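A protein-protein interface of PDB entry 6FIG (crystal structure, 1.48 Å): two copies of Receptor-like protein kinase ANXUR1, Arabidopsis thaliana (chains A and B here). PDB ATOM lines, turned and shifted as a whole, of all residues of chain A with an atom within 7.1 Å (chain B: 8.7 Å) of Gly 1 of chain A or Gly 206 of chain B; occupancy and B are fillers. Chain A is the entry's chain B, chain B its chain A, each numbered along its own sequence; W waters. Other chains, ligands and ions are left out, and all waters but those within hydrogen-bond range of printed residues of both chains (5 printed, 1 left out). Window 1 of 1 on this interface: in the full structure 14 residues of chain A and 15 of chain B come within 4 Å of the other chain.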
ATOM      1  N   GLY A   1      25.638 -26.482   5.426  1.00  0.00           N
ATOM      2  CA  GLY A   1      25.369 -26.881   3.986  1.00  0.00           C
ATOM      3  C   GLY A   1      25.752 -28.309   3.686  1.00  0.00           C
ATOM      4  O   GLY A   1      25.104 -29.000   2.870  1.00  0.00           O
ATOM      5  N   GLN A   2      26.853 -28.716   4.322  1.00  0.00           N
ATOM      6  CA  GLN A   2      27.297 -30.089   4.506  1.00  0.00           C
ATOM      7  C   GLN A   2      28.414 -30.284   3.507  1.00  0.00           C
ATOM      8  O   GLN A   2      28.669 -29.414   2.668  1.00  0.00           O
ATOM      9  CB  GLN A   2      26.186 -31.123   4.356  1.00  0.00           C
ATOM     10  CG  GLN A   2      26.398 -32.421   5.124  1.00  0.00           C
ATOM     11  CD  GLN A   2      26.010 -32.361   6.594  1.00  0.00           C
ATOM     12  OE1 GLN A   2      25.067 -31.684   6.997  1.00  0.00           O
ATOM     13  NE2 GLN A   2      26.752 -33.098   7.405  1.00  0.00           N
ATOM     14  N   ASP A   3      29.069 -31.425   3.590  1.00  0.00           N
ATOM     15  CA  ASP A   3      30.271 -31.653   2.818  1.00  0.00           C
ATOM     16  C   ASP A   3      29.946 -31.673   1.340  1.00  0.00           C
ATOM     17  O   ASP A   3      28.888 -32.164   0.938  1.00  0.00           O
ATOM     18  CB  ASP A   3      30.930 -32.982   3.194  1.00  0.00           C
ATOM     19  CG  ASP A   3      31.424 -33.021   4.641  1.00  0.00           C
ATOM     20  OD1 ASP A   3      31.455 -31.974   5.335  1.00  0.00           O
ATOM     21  OD2 ASP A   3      31.827 -34.120   5.058  1.00  0.00           O
ATOM     22  N   LEU A   4      30.897 -31.195   0.548  1.00  0.00           N
ATOM     23  CA  LEU A   4      30.726 -31.086  -0.891  1.00  0.00           C
ATOM     24  C   LEU A   4      31.938 -31.615  -1.621  1.00  0.00           C
ATOM     25  O   LEU A   4      33.070 -31.433  -1.159  1.00  0.00           O
ATOM     26  CB  LEU A   4      30.565 -29.627  -1.306  1.00  0.00           C
ATOM     27  CG  LEU A   4      29.400 -28.800  -0.823  1.00  0.00           C
ATOM     28  CD1 LEU A   4      29.534 -27.411  -1.441  1.00  0.00           C
ATOM     29  CD2 LEU A   4      28.084 -29.461  -1.200  1.00  0.00           C
ATOM     30  N   PHE A  28      27.293 -22.967  -6.532  1.00  0.00           N
ATOM     31  CA  PHE A  28      28.047 -22.345  -5.444  1.00  0.00           C
ATOM     32  C   PHE A  28      28.871 -21.167  -5.911  1.00  0.00           C
ATOM     33  O   PHE A  28      29.502 -20.474  -5.111  1.00  0.00           O
ATOM     34  CB  PHE A  28      28.938 -23.414  -4.780  1.00  0.00           C
ATOM     35  CG  PHE A  28      28.149 -24.545  -4.230  1.00  0.00           C
ATOM     36  CD1 PHE A  28      27.529 -24.424  -2.996  1.00  0.00           C
ATOM     37  CD2 PHE A  28      27.936 -25.695  -4.974  1.00  0.00           C
ATOM     38  CE1 PHE A  28      26.765 -25.461  -2.485  1.00  0.00           C
ATOM     39  CE2 PHE A  28      27.158 -26.720  -4.490  1.00  0.00           C
ATOM     40  CZ  PHE A  28      26.576 -26.612  -3.236  1.00  0.00           C
ATOM     41  N   ILE A  66      30.458 -21.308  -0.117  1.00  0.00           N
ATOM     42  CA  ILE A  66      30.086 -22.659   0.255  1.00  0.00           C
ATOM     43  C   ILE A  66      29.530 -22.612   1.684  1.00  0.00           C
ATOM     44  O   ILE A  66      30.224 -22.188   2.591  1.00  0.00           O
ATOM     45  CB  ILE A  66      31.295 -23.607   0.115  1.00  0.00           C
ATOM     46  CG1 ILE A  66      31.640 -23.723  -1.394  1.00  0.00           C
ATOM     47  CG2 ILE A  66      30.985 -24.975   0.732  1.00  0.00           C
ATOM     48  CD1 ILE A  66      32.852 -24.525  -1.755  1.00  0.00           C
ATOM     49  N   PRO A  67      28.272 -23.039   1.886  1.00  0.00           N
ATOM     50  CA  PRO A  67      27.743 -23.070   3.235  1.00  0.00           C
ATOM     51  C   PRO A  67      28.525 -24.041   4.098  1.00  0.00           C
ATOM     52  O   PRO A  67      28.781 -25.165   3.686  1.00  0.00           O
ATOM     53  CB  PRO A  67      26.292 -23.547   3.049  1.00  0.00           C
ATOM     54  CG  PRO A  67      25.974 -23.198   1.644  1.00  0.00           C
ATOM     55  CD  PRO A  67      27.238 -23.421   0.909  1.00  0.00           C
ATOM     56  N   ILE A  68      28.891 -23.574   5.286  1.00  0.00           N
ATOM     57  CA  ILE A  68      29.631 -24.384   6.249  1.00  0.00           C
ATOM     58  C   ILE A  68      29.095 -24.114   7.651  1.00  0.00           C
ATOM     59  O   ILE A  68      28.293 -23.232   7.860  1.00  0.00           O
ATOM     60  CB  ILE A  68      31.159 -24.091   6.248  1.00  0.00           C
ATOM     61  CG1 ILE A  68      31.436 -22.603   6.473  1.00  0.00           C
ATOM     62  CG2 ILE A  68      31.822 -24.634   4.998  1.00  0.00           C
ATOM     63  CD1 ILE A  68      32.871 -22.319   6.863  1.00  0.00           C
ATOM     64  N   LYS A  69      29.591 -24.885   8.612  1.00  0.00           N
ATOM     65  CA  LYS A  69      29.334 -24.630  10.024  1.00  0.00           C
ATOM     66  C   LYS A  69      30.511 -23.834  10.616  1.00  0.00           C
ATOM     67  O   LYS A  69      31.660 -24.311  10.617  1.00  0.00           O
ATOM     68  CB  LYS A  69      29.155 -25.943  10.758  1.00  0.00           C
ATOM     69  CG  LYS A  69      28.542 -25.742  12.108  1.00  0.00           C
ATOM     70  CD  LYS A  69      27.895 -27.008  12.650  1.00  0.00           C
ATOM     71  CE  LYS A  69      26.947 -26.695  13.765  1.00  0.00           C
ATOM     72  NZ  LYS A  69      27.619 -26.283  15.034  1.00  0.00           N
ATOM     73  N   GLY A  70      30.204 -22.641  11.110  1.00  0.00           N
ATOM     74  CA  GLY A  70      31.202 -21.661  11.562  1.00  0.00           C
ATOM     75  C   GLY A  70      32.148 -22.089  12.668  1.00  0.00           C
ATOM     76  O   GLY A  70      33.312 -21.665  12.694  1.00  0.00           O
ATOM     77  N   LYS A  72      33.336 -25.071  13.226  1.00  0.00           N
ATOM     78  CA  LYS A  72      34.063 -26.267  12.864  1.00  0.00           C
ATOM     79  C   LYS A  72      35.283 -25.993  12.005  1.00  0.00           C
ATOM     80  O   LYS A  72      35.322 -25.014  11.218  1.00  0.00           O
ATOM     81  CB  LYS A  72      33.166 -27.224  12.074  1.00  0.00           C
ATOM     82  CG  LYS A  72      31.917 -27.686  12.803  1.00  0.00           C
ATOM     83  CD  LYS A  72      32.169 -28.923  13.616  1.00  0.00           C
ATOM     84  CE  LYS A  72      30.858 -29.594  13.996  1.00  0.00           C
ATOM     85  NZ  LYS A  72      31.135 -30.943  14.540  1.00  0.00           N
ATOM     86  N   ASP A 134      29.219 -18.712   8.512  1.00  0.00           N
ATOM     87  CA  ASP A 134      28.521 -19.875   7.921  1.00  0.00           C
ATOM     88  C   ASP A 134      28.682 -20.003   6.410  1.00  0.00           C
ATOM     89  O   ASP A 134      28.038 -20.842   5.794  1.00  0.00           O
ATOM     90  CB  ASP A 134      27.057 -19.910   8.357  1.00  0.00           C
ATOM     91  CG  ASP A 134      26.301 -18.671   7.963  1.00  0.00           C
ATOM     92  OD1 ASP A 134      26.875 -17.838   7.218  1.00  0.00           O
ATOM     93  OD2 ASP A 134      25.144 -18.499   8.408  1.00  0.00           O
ATOM     94  N   GLN A 160      33.967 -31.254   6.602  1.00  0.00           N
ATOM     95  CA  GLN A 160      34.065 -30.938   8.014  1.00  0.00           C
ATOM     96  C   GLN A 160      34.993 -31.939   8.690  1.00  0.00           C
ATOM     97  O   GLN A 160      34.931 -33.140   8.393  1.00  0.00           O
ATOM     98  CB  GLN A 160      32.664 -31.014   8.613  1.00  0.00           C
ATOM     99  CG  GLN A 160      32.403 -30.054   9.710  1.00  0.00           C
ATOM    100  CD  GLN A 160      31.014 -30.295  10.254  1.00  0.00           C
ATOM    101  OE1 GLN A 160      30.047 -29.643   9.841  1.00  0.00           O
ATOM    102  NE2 GLN A 160      30.901 -31.290  11.135  1.00  0.00           N
ATOM    103  N   ASP B   3      30.088 -30.446  18.963  1.00  0.00           N
ATOM    104  CA  ASP B   3      28.750 -30.985  18.721  1.00  0.00           C
ATOM    105  C   ASP B   3      28.763 -32.500  18.934  1.00  0.00           C
ATOM    106  O   ASP B   3      29.747 -33.160  18.608  1.00  0.00           O
ATOM    107  CB  ASP B   3      28.268 -30.692  17.304  1.00  0.00           C
ATOM    108  CG  ASP B   3      28.148 -29.204  16.999  1.00  0.00           C
ATOM    109  OD1 ASP B   3      28.077 -28.377  17.927  1.00  0.00           O
ATOM    110  OD2 ASP B   3      28.112 -28.884  15.803  1.00  0.00           O
ATOM    111  N   LYS B  20      24.676 -39.390   9.081  1.00  0.00           N
ATOM    112  CA  LYS B  20      25.021 -38.741  10.335  1.00  0.00           C
ATOM    113  C   LYS B  20      25.782 -39.752  11.194  1.00  0.00           C
ATOM    114  O   LYS B  20      25.348 -40.897  11.304  1.00  0.00           O
ATOM    115  CB  LYS B  20      23.768 -38.298  11.077  1.00  0.00           C
ATOM    116  CG  LYS B  20      24.018 -37.574  12.395  1.00  0.00           C
ATOM    117  CD  LYS B  20      22.708 -37.137  13.040  1.00  0.00           C
ATOM    118  CE  LYS B  20      22.153 -35.868  12.415  1.00  0.00           C
ATOM    119  NZ  LYS B  20      22.703 -34.621  12.998  1.00  0.00           N
ATOM    120  N   LEU B  75      21.124 -26.070  19.652  1.00  0.00           N
ATOM    121  CA  LEU B  75      20.053 -26.997  19.381  1.00  0.00           C
ATOM    122  C   LEU B  75      20.238 -28.236  20.239  1.00  0.00           C
ATOM    123  O   LEU B  75      21.362 -28.755  20.371  1.00  0.00           O
ATOM    124  CB  LEU B  75      20.028 -27.452  17.929  1.00  0.00           C
ATOM    125  CG  LEU B  75      19.504 -26.530  16.886  1.00  0.00           C
ATOM    126  CD1 LEU B  75      19.626 -27.134  15.495  1.00  0.00           C
ATOM    127  CD2 LEU B  75      18.063 -26.094  17.149  1.00  0.00           C
ATOM    128  N   ARG B  77      18.375 -31.995  20.564  1.00  0.00           N
ATOM    129  CA  ARG B  77      17.394 -32.935  20.089  1.00  0.00           C
ATOM    130  C   ARG B  77      17.350 -34.172  20.960  1.00  0.00           C
ATOM    131  O   ARG B  77      18.399 -34.688  21.344  1.00  0.00           O
ATOM    132  CB  ARG B  77      17.690 -33.398  18.672  1.00  0.00           C
ATOM    133  CG  ARG B  77      17.584 -32.288  17.658  1.00  0.00           C
ATOM    134  CD  ARG B  77      17.936 -32.756  16.278  1.00  0.00           C
ATOM    135  NE  ARG B  77      17.921 -31.619  15.369  1.00  0.00           N
ATOM    136  CZ  ARG B  77      18.795 -31.399  14.394  1.00  0.00           C
ATOM    137  NH1 ARG B  77      19.800 -32.221  14.145  1.00  0.00           N
ATOM    138  NH2 ARG B  77      18.680 -30.296  13.664  1.00  0.00           N
ATOM    139  N   GLU B 157      21.206 -35.151  20.603  1.00  0.00           N
ATOM    140  CA  GLU B 157      22.143 -34.263  19.902  1.00  0.00           C
ATOM    141  C   GLU B 157      22.213 -32.907  20.566  1.00  0.00           C
ATOM    142  O   GLU B 157      21.195 -32.376  21.009  1.00  0.00           O
ATOM    143  CB  GLU B 157      21.793 -34.033  18.435  1.00  0.00           C
ATOM    144  CG  GLU B 157      21.767 -35.239  17.546  1.00  0.00           C
ATOM    145  CD  GLU B 157      21.635 -34.796  16.102  1.00  0.00           C
ATOM    146  OE1 GLU B 157      20.496 -34.694  15.629  1.00  0.00           O
ATOM    147  OE2 GLU B 157      22.681 -34.497  15.486  1.00  0.00           O
ATOM    148  N   ILE B 159      24.052 -29.280  19.444  1.00  0.00           N
ATOM    149  CA  ILE B 159      24.639 -28.649  18.262  1.00  0.00           C
ATOM    150  C   ILE B 159      24.696 -27.150  18.528  1.00  0.00           C
ATOM    151  O   ILE B 159      23.648 -26.517  18.695  1.00  0.00           O
ATOM    152  CB  ILE B 159      23.757 -28.901  17.027  1.00  0.00           C
ATOM    153  CG1 ILE B 159      23.581 -30.412  16.755  1.00  0.00           C
ATOM    154  CG2 ILE B 159      24.319 -28.204  15.797  1.00  0.00           C
ATOM    155  CD1 ILE B 159      22.334 -30.748  15.977  1.00  0.00           C
ATOM    156  N   GLN B 160      25.888 -26.587  18.546  1.00  0.00           N
ATOM    157  CA  GLN B 160      26.041 -25.134  18.635  1.00  0.00           C
ATOM    158  C   GLN B 160      25.409 -24.472  17.407  1.00  0.00           C
ATOM    159  O   GLN B 160      25.602 -24.941  16.285  1.00  0.00           O
ATOM    160  CB  GLN B 160      27.512 -24.744  18.717  1.00  0.00           C
ATOM    161  CG  GLN B 160      27.713 -23.304  19.120  1.00  0.00           C
ATOM    162  CD  GLN B 160      29.160 -22.931  19.217  1.00  0.00           C
ATOM    163  OE1 GLN B 160      29.892 -23.472  20.058  1.00  0.00           O
ATOM    164  NE2 GLN B 160      29.582 -21.995  18.376  1.00  0.00           N
ATOM    165  N   MET B 161      24.640 -23.396  17.603  1.00  0.00           N
ATOM    166  CA  MET B 161      23.962 -22.732  16.485  1.00  0.00           C
ATOM    167  C   MET B 161      24.087 -21.233  16.614  1.00  0.00           C
ATOM    168  O   MET B 161      24.273 -20.720  17.692  1.00  0.00           O
ATOM    169  CB  MET B 161      22.502 -23.145  16.367  1.00  0.00           C
ATOM    170  CG  MET B 161      21.638 -22.667  17.514  1.00  0.00           C
ATOM    171  SD  MET B 161      19.923 -23.059  17.304  1.00  0.00           S
ATOM    172  CE  MET B 161      19.446 -21.899  16.039  1.00  0.00           C
ATOM    173  N   PRO B 162      24.014 -20.518  15.491  1.00  0.00           N
ATOM    174  CA  PRO B 162      23.987 -19.064  15.575  1.00  0.00           C
ATOM    175  C   PRO B 162      22.689 -18.520  16.209  1.00  0.00           C
ATOM    176  O   PRO B 162      21.692 -19.236  16.388  1.00  0.00           O
ATOM    177  CB  PRO B 162      24.058 -18.616  14.088  1.00  0.00           C
ATOM    178  CG  PRO B 162      24.465 -19.831  13.324  1.00  0.00           C
ATOM    179  CD  PRO B 162      23.945 -20.999  14.099  1.00  0.00           C
ATOM    180  N   ILE B 198      13.607 -31.979   2.671  1.00  0.00           N
ATOM    181  CA  ILE B 198      15.035 -31.724   2.662  1.00  0.00           C
ATOM    182  C   ILE B 198      15.622 -32.455   3.876  1.00  0.00           C
ATOM    183  O   ILE B 198      15.307 -32.068   5.008  1.00  0.00           O
ATOM    184  CB  ILE B 198      15.350 -30.223   2.793  1.00  0.00           C
ATOM    185  CG1 ILE B 198      14.693 -29.428   1.665  1.00  0.00           C
ATOM    186  CG2 ILE B 198      16.858 -30.001   2.775  1.00  0.00           C
ATOM    187  CD1 ILE B 198      14.811 -27.925   1.821  1.00  0.00           C
ATOM    188  N   PRO B 199      16.480 -33.473   3.649  1.00  0.00           N
ATOM    189  CA  PRO B 199      17.102 -34.207   4.760  1.00  0.00           C
ATOM    190  C   PRO B 199      18.136 -33.333   5.456  1.00  0.00           C
ATOM    191  O   PRO B 199      18.653 -32.377   4.861  1.00  0.00           O
ATOM    192  CB  PRO B 199      17.777 -35.391   4.077  1.00  0.00           C
ATOM    193  CG  PRO B 199      18.134 -34.864   2.729  1.00  0.00           C
ATOM    194  CD  PRO B 199      17.042 -33.898   2.348  1.00  0.00           C
ATOM    195  N   GLY B 200      18.424 -33.658   6.711  1.00  0.00           N
ATOM    196  CA  GLY B 200      19.409 -32.907   7.500  1.00  0.00           C
ATOM    197  C   GLY B 200      20.771 -32.777   6.831  1.00  0.00           C
ATOM    198  O   GLY B 200      21.436 -31.747   6.935  1.00  0.00           O
ATOM    199  N   SER B 201      21.179 -33.789   6.076  1.00  0.00           N
ATOM    200  CA  SER B 201      22.445 -33.723   5.354  1.00  0.00           C
ATOM    201  C   SER B 201      22.526 -32.582   4.333  1.00  0.00           C
ATOM    202  O   SER B 201      23.604 -32.209   3.905  1.00  0.00           O
ATOM    203  CB  SER B 201      22.723 -35.065   4.662  1.00  0.00           C
ATOM    204  OG  SER B 201      21.733 -35.309   3.673  1.00  0.00           O
ATOM    205  N   GLN B 202      21.385 -32.065   3.887  1.00  0.00           N
ATOM    206  CA  GLN B 202      21.351 -30.969   2.926  1.00  0.00           C
ATOM    207  C   GLN B 202      21.030 -29.611   3.560  1.00  0.00           C
ATOM    208  O   GLN B 202      20.953 -28.606   2.866  1.00  0.00           O
ATOM    209  CB  GLN B 202      20.344 -31.296   1.822  1.00  0.00           C
ATOM    210  CG  GLN B 202      20.843 -32.402   0.902  1.00  0.00           C
ATOM    211  CD  GLN B 202      22.001 -31.928   0.029  1.00  0.00           C
ATOM    212  OE1 GLN B 202      21.976 -30.806  -0.508  1.00  0.00           O
ATOM    213  NE2 GLN B 202      23.008 -32.762  -0.119  1.00  0.00           N
ATOM    214  N   ASP B 203      20.873 -29.586   4.873  1.00  0.00           N
ATOM    215  CA  ASP B 203      20.537 -28.348   5.584  1.00  0.00           C
ATOM    216  C   ASP B 203      21.727 -27.406   5.599  1.00  0.00           C
ATOM    217  O   ASP B 203      22.879 -27.863   5.561  1.00  0.00           O
ATOM    218  CB  ASP B 203      20.130 -28.667   7.017  1.00  0.00           C
ATOM    219  CG  ASP B 203      19.612 -27.461   7.762  1.00  0.00           C
ATOM    220  OD1 ASP B 203      18.992 -26.563   7.114  1.00  0.00           O
ATOM    221  OD2 ASP B 203      19.764 -27.411   8.989  1.00  0.00           O
ATOM    222  N   SER B 204      21.457 -26.100   5.667  1.00  0.00           N
ATOM    223  CA  SER B 204      22.509 -25.092   5.765  1.00  0.00           C
ATOM    224  C   SER B 204      22.967 -24.912   7.208  1.00  0.00           C
ATOM    225  O   SER B 204      22.390 -25.476   8.128  1.00  0.00           O
ATOM    226  CB  SER B 204      22.032 -23.759   5.208  1.00  0.00           C
ATOM    227  OG  SER B 204      20.890 -23.323   5.907  1.00  0.00           O
ATOM    228  N   GLY B 205      24.058 -24.159   7.379  1.00  0.00           N
ATOM    229  CA  GLY B 205      24.590 -23.905   8.734  1.00  0.00           C
ATOM    230  C   GLY B 205      25.210 -25.115   9.415  1.00  0.00           C
ATOM    231  O   GLY B 205      25.489 -25.076  10.596  1.00  0.00           O
ATOM    232  N   GLY B 206      25.390 -26.207   8.674  1.00  0.00           N
ATOM    233  CA  GLY B 206      25.622 -27.541   9.274  1.00  0.00           C
ATOM    234  C   GLY B 206      24.680 -27.954  10.401  1.00  0.00           C
ATOM    235  O   GLY B 206      25.069 -28.737  11.268  1.00  0.00           O
ATOM    236  N   LEU B 207      23.429 -27.467  10.393  1.00  0.00           N
ATOM    237  CA  LEU B 207      22.539 -27.648  11.528  1.00  0.00           C
ATOM    238  C   LEU B 207      21.697 -28.930  11.456  1.00  0.00           C
ATOM    239  O   LEU B 207      20.974 -29.243  12.377  1.00  0.00           O
ATOM    240  CB  LEU B 207      21.627 -26.423  11.699  1.00  0.00           C
ATOM    241  CG  LEU B 207      22.331 -25.109  12.029  1.00  0.00           C
ATOM    242  CD1 LEU B 207      21.312 -23.971  12.071  1.00  0.00           C
ATOM    243  CD2 LEU B 207      23.079 -25.228  13.352  1.00  0.00           C
ATOM    244  N   THR B 208      21.801 -29.649  10.336  1.00  0.00           N
ATOM    245  CA  THR B 208      21.078 -30.900  10.106  1.00  0.00           C
ATOM    246  C   THR B 208      19.598 -30.932  10.459  1.00  0.00           C
ATOM    247  O   THR B 208      19.060 -31.965  10.859  1.00  0.00           O
ATOM    248  CB  THR B 208      21.830 -32.148  10.667  1.00  0.00           C
ATOM    249  OG1 THR B 208      21.933 -32.094  12.101  1.00  0.00           O
ATOM    250  CG2 THR B 208      23.187 -32.282  10.041  1.00  0.00           C
ATOM    251  N   ARG B 209      18.930 -29.793  10.257  1.00  0.00           N
ATOM    252  CA  ARG B 209      17.480 -29.703  10.358  1.00  0.00           C
ATOM    253  C   ARG B 209      16.827 -30.370   9.150  1.00  0.00           C
ATOM    254  O   ARG B 209      17.294 -30.229   8.022  1.00  0.00           O
ATOM    255  CB  ARG B 209      17.012 -28.252  10.378  1.00  0.00           C
ATOM    256  CG  ARG B 209      17.513 -27.443  11.559  1.00  0.00           C
ATOM    257  CD  ARG B 209      17.378 -25.942  11.319  1.00  0.00           C
ATOM    258  NE  ARG B 209      18.193 -25.525  10.197  1.00  0.00           N
ATOM    259  CZ  ARG B 209      18.380 -24.265   9.794  1.00  0.00           C
ATOM    260  NH1 ARG B 209      17.804 -23.241  10.410  1.00  0.00           N
ATOM    261  NH2 ARG B 209      19.128 -24.044   8.724  1.00  0.00           N
ATOM    262  N   VAL B 242      23.111 -17.556   5.631  1.00  0.00           N
ATOM    263  CA  VAL B 242      22.716 -18.793   4.955  1.00  0.00           C
ATOM    264  C   VAL B 242      22.195 -19.835   5.934  1.00  0.00           C
ATOM    265  O   VAL B 242      21.400 -20.675   5.549  1.00  0.00           O
ATOM    266  CB  VAL B 242      23.823 -19.409   4.034  1.00  0.00           C
ATOM    267  CG1 VAL B 242      24.217 -18.415   2.951  1.00  0.00           C
ATOM    268  CG2 VAL B 242      24.998 -19.922   4.799  1.00  0.00           C
ATOM    269  N   SER B 243      22.610 -19.755   7.211  1.00  0.00           N
ATOM    270  CA  SER B 243      22.089 -20.635   8.255  1.00  0.00           C
ATOM    271  C   SER B 243      20.597 -20.510   8.508  1.00  0.00           C
ATOM    272  O   SER B 243      19.998 -21.402   9.118  1.00  0.00           O
ATOM    273  CB  SER B 243      22.798 -20.405   9.602  1.00  0.00           C
ATOM    274  OG  SER B 243      24.169 -20.661   9.498  1.00  0.00           O
ATOM    275  N   ALA B 245      18.119 -20.759   6.390  1.00  0.00           N
ATOM    276  CA  ALA B 245      17.452 -21.872   5.689  1.00  0.00           C
ATOM    277  C   ALA B 245      18.246 -22.169   4.425  1.00  0.00           C
ATOM    278  O   ALA B 245      18.828 -21.259   3.840  1.00  0.00           O
ATOM    279  CB  ALA B 245      16.030 -21.509   5.320  1.00  0.00           C
ATOM    280  N   PRO B 246      18.271 -23.435   4.003  1.00  0.00           N
ATOM    281  CA  PRO B 246      19.014 -23.792   2.816  1.00  0.00           C
ATOM    282  C   PRO B 246      18.376 -23.309   1.525  1.00  0.00           C
ATOM    283  O   PRO B 246      17.160 -23.027   1.454  1.00  0.00           O
ATOM    284  CB  PRO B 246      19.037 -25.329   2.863  1.00  0.00           C
ATOM    285  CG  PRO B 246      17.830 -25.688   3.622  1.00  0.00           C
ATOM    286  CD  PRO B 246      17.645 -24.602   4.634  1.00  0.00           C
ATOM    287  N   ALA B 247      19.203 -23.201   0.499  1.00  0.00           N
ATOM    288  CA  ALA B 247      18.765 -22.604  -0.770  1.00  0.00           C
ATOM    289  C   ALA B 247      17.554 -23.302  -1.362  1.00  0.00           C
ATOM    290  O   ALA B 247      16.676 -22.648  -1.945  1.00  0.00           O
ATOM    291  CB  ALA B 247      19.891 -22.584  -1.778  1.00  0.00           C
HETATM  292  O   HOH W   1      25.833 -16.110   5.627  1.00  0.00           O
HETATM  293  O   HOH W   2      31.465 -28.840  17.003  1.00  0.00           O
HETATM  294  O   HOH W   3      26.016 -22.751   6.165  1.00  0.00           O
HETATM  295  O   HOH W   4      27.422 -30.203  11.181  1.00  0.00           O
HETATM  296  O   HOH W   5      27.870 -30.702  13.913  1.00  0.00           O
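The backbone NH (N) of Gly 1 of chain A sits close to the backbone NH (N) of Gly 206 of chain B, at 3.3 Å.
The side-chain carboxylate (OD2) of Asp 3 of chain B is in salt-bridge range of the side-chain amino group (NZ) of Lys 69 of chain A (2.8 Å).
N of Gly 1 of chain A lies close to N of Gly 205 of chain B.
The side-chain amino group (NZ) of Lys 72 of chain A lies within salt-bridge range of the side-chain carboxylate (OD2) of Asp 3 of chain B, 3.9 Å away.
The side-chain carboxylate (OD2) of Asp 134 of chain A is in hydrogen-bond range of the side-chain hydroxyl (OG) of Ser 243 of chain B, at 2.6 Å.
O of Asp 203 of chain B sits at hydrogen-bond distance from N of Gly 1 of chain A (3.1 Å).
O of Gln 160 of chain B sits at hydrogen-bond distance from NZ of Lys 69 of chain A (2.7 Å).
The backbone carbonyl oxygen of Ser 201 of chain B sits close to the side-chain amide oxygen of Gln 2 of chain A, 3.5 Å away.
The guanidinium group (NH2) of Arg 209 of chain B is in hydrogen-bond range of the side-chain hydroxyl (OG) of Ser 204 of chain B, 3.4 Å away.
The side-chain carboxylate (OD2) of Asp 203 of chain B is in salt-bridge range of the guanidinium group (NE) of Arg 209 of chain B.
The guanidinium group of Arg 77 of chain B is in hydrogen-bond range of the side-chain hydroxyl of Thr 208 of chain B.
O of Ser 243 of chain B lies within hydrogen-bond range of NH2 of Arg 209 of chain B.
Gly 1 of chain A touches just these residues of chain B: Ser 201, Asp 203, Ser 204, Gly 205 and Gly 206.
Gly 206 of chain B touches two residues of chain A.
Of chain A, only Gly 1, Ile 68 and Lys 69 come within 4 Å of Gly 205 of chain B.
Of the printed residues of chain A, Ile 159 of chain B touches Lys 69.
Printed residues of chain B within 4 Å of Gln 2 of chain A: Gly 200, Ser 201 and Thr 208.
Printed residues of chain A within 4 Å of Gln 160 of chain B: Lys 69 (2.7 Å).
Printed residues of chain B within 4 Å of Ile 68 of chain A: Gly 205 (3.9 Å).
Of the printed residues of chain B, Lys 72 of chain A touches Asp 3 (3.4 Å).
Gly 70 of chain A touches none of the printed residues of chain B.
Ile 66 of chain A touches none of the printed residues of chain B.
The nearest residue of chain B that does not touch Gly 1 of chain A is Gln 202 of chain B (4.2 Å).
The nearest residue of chain A that does not touch Gly 206 of chain B is Ile 68 of chain A (4.2 Å).
2 positions are printed for both chains.
Of the 17 pairs that touch across the chains among the printed residues, none has its exchanged pair printed and touching as well.
Among the printed residues, merely in contact across the chains: Asp 134 of chain A with Val 242 of chain B (3.3 Å), Gly 1 of chain A with Ser 204 of chain B (3.4 Å), Lys 69 of chain A with Gly 205 of chain B (3.5 Å), Lys 69 of chain A with Gly 206 of chain B (3.6 Å), Gln 2 of chain A with Thr 208 of chain B (3.6 Å), Gln 2 of chain A with Gly 200 of chain B (3.6 Å), Lys 69 of chain A with Ile 159 of chain B (3.6 Å), Gly 1 of chain A with Ser 201 of chain B (3.7 Å) and Ile 68 of chain A with Gly 205 of chain B (3.9 Å).
Among the printed residues, Asp or Glu carboxylates within 4 Å of a Lys or Arg side-chain nitrogen of the other chain: Lys 69 of chain A with Asp 3 of chain B (2.8 Å) and Lys 72 of chain A with Asp 3 of chain B (3.9 Å).
Water W1 lies within hydrogen-bond range of the side-chain carboxylate of Asp 134 of chain A (2.6 Å) and the backbone NH of Val 242 of chain B (3.1 Å).
Water W5 bridges OD2 of Asp 3 of chain B (2.6 Å) and NZ of Lys 72 of chain A (3.3 Å).
Water W3 lies within hydrogen-bond range of N of Gly 205 of chain B (2.7 Å), O of Asp 134 of chain A (2.8 Å) and O of Ile 68 of chain A (2.9 Å).
Water W4 lies within hydrogen-bond range of O of Gly 206 of chain B and OE1 of Gln 160 of chain A.
Water W2 bridges the backbone NH of Asp 3 of chain B (2.9 Å) and the side-chain amino group of Lys 72 of chain A (3.3 Å).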
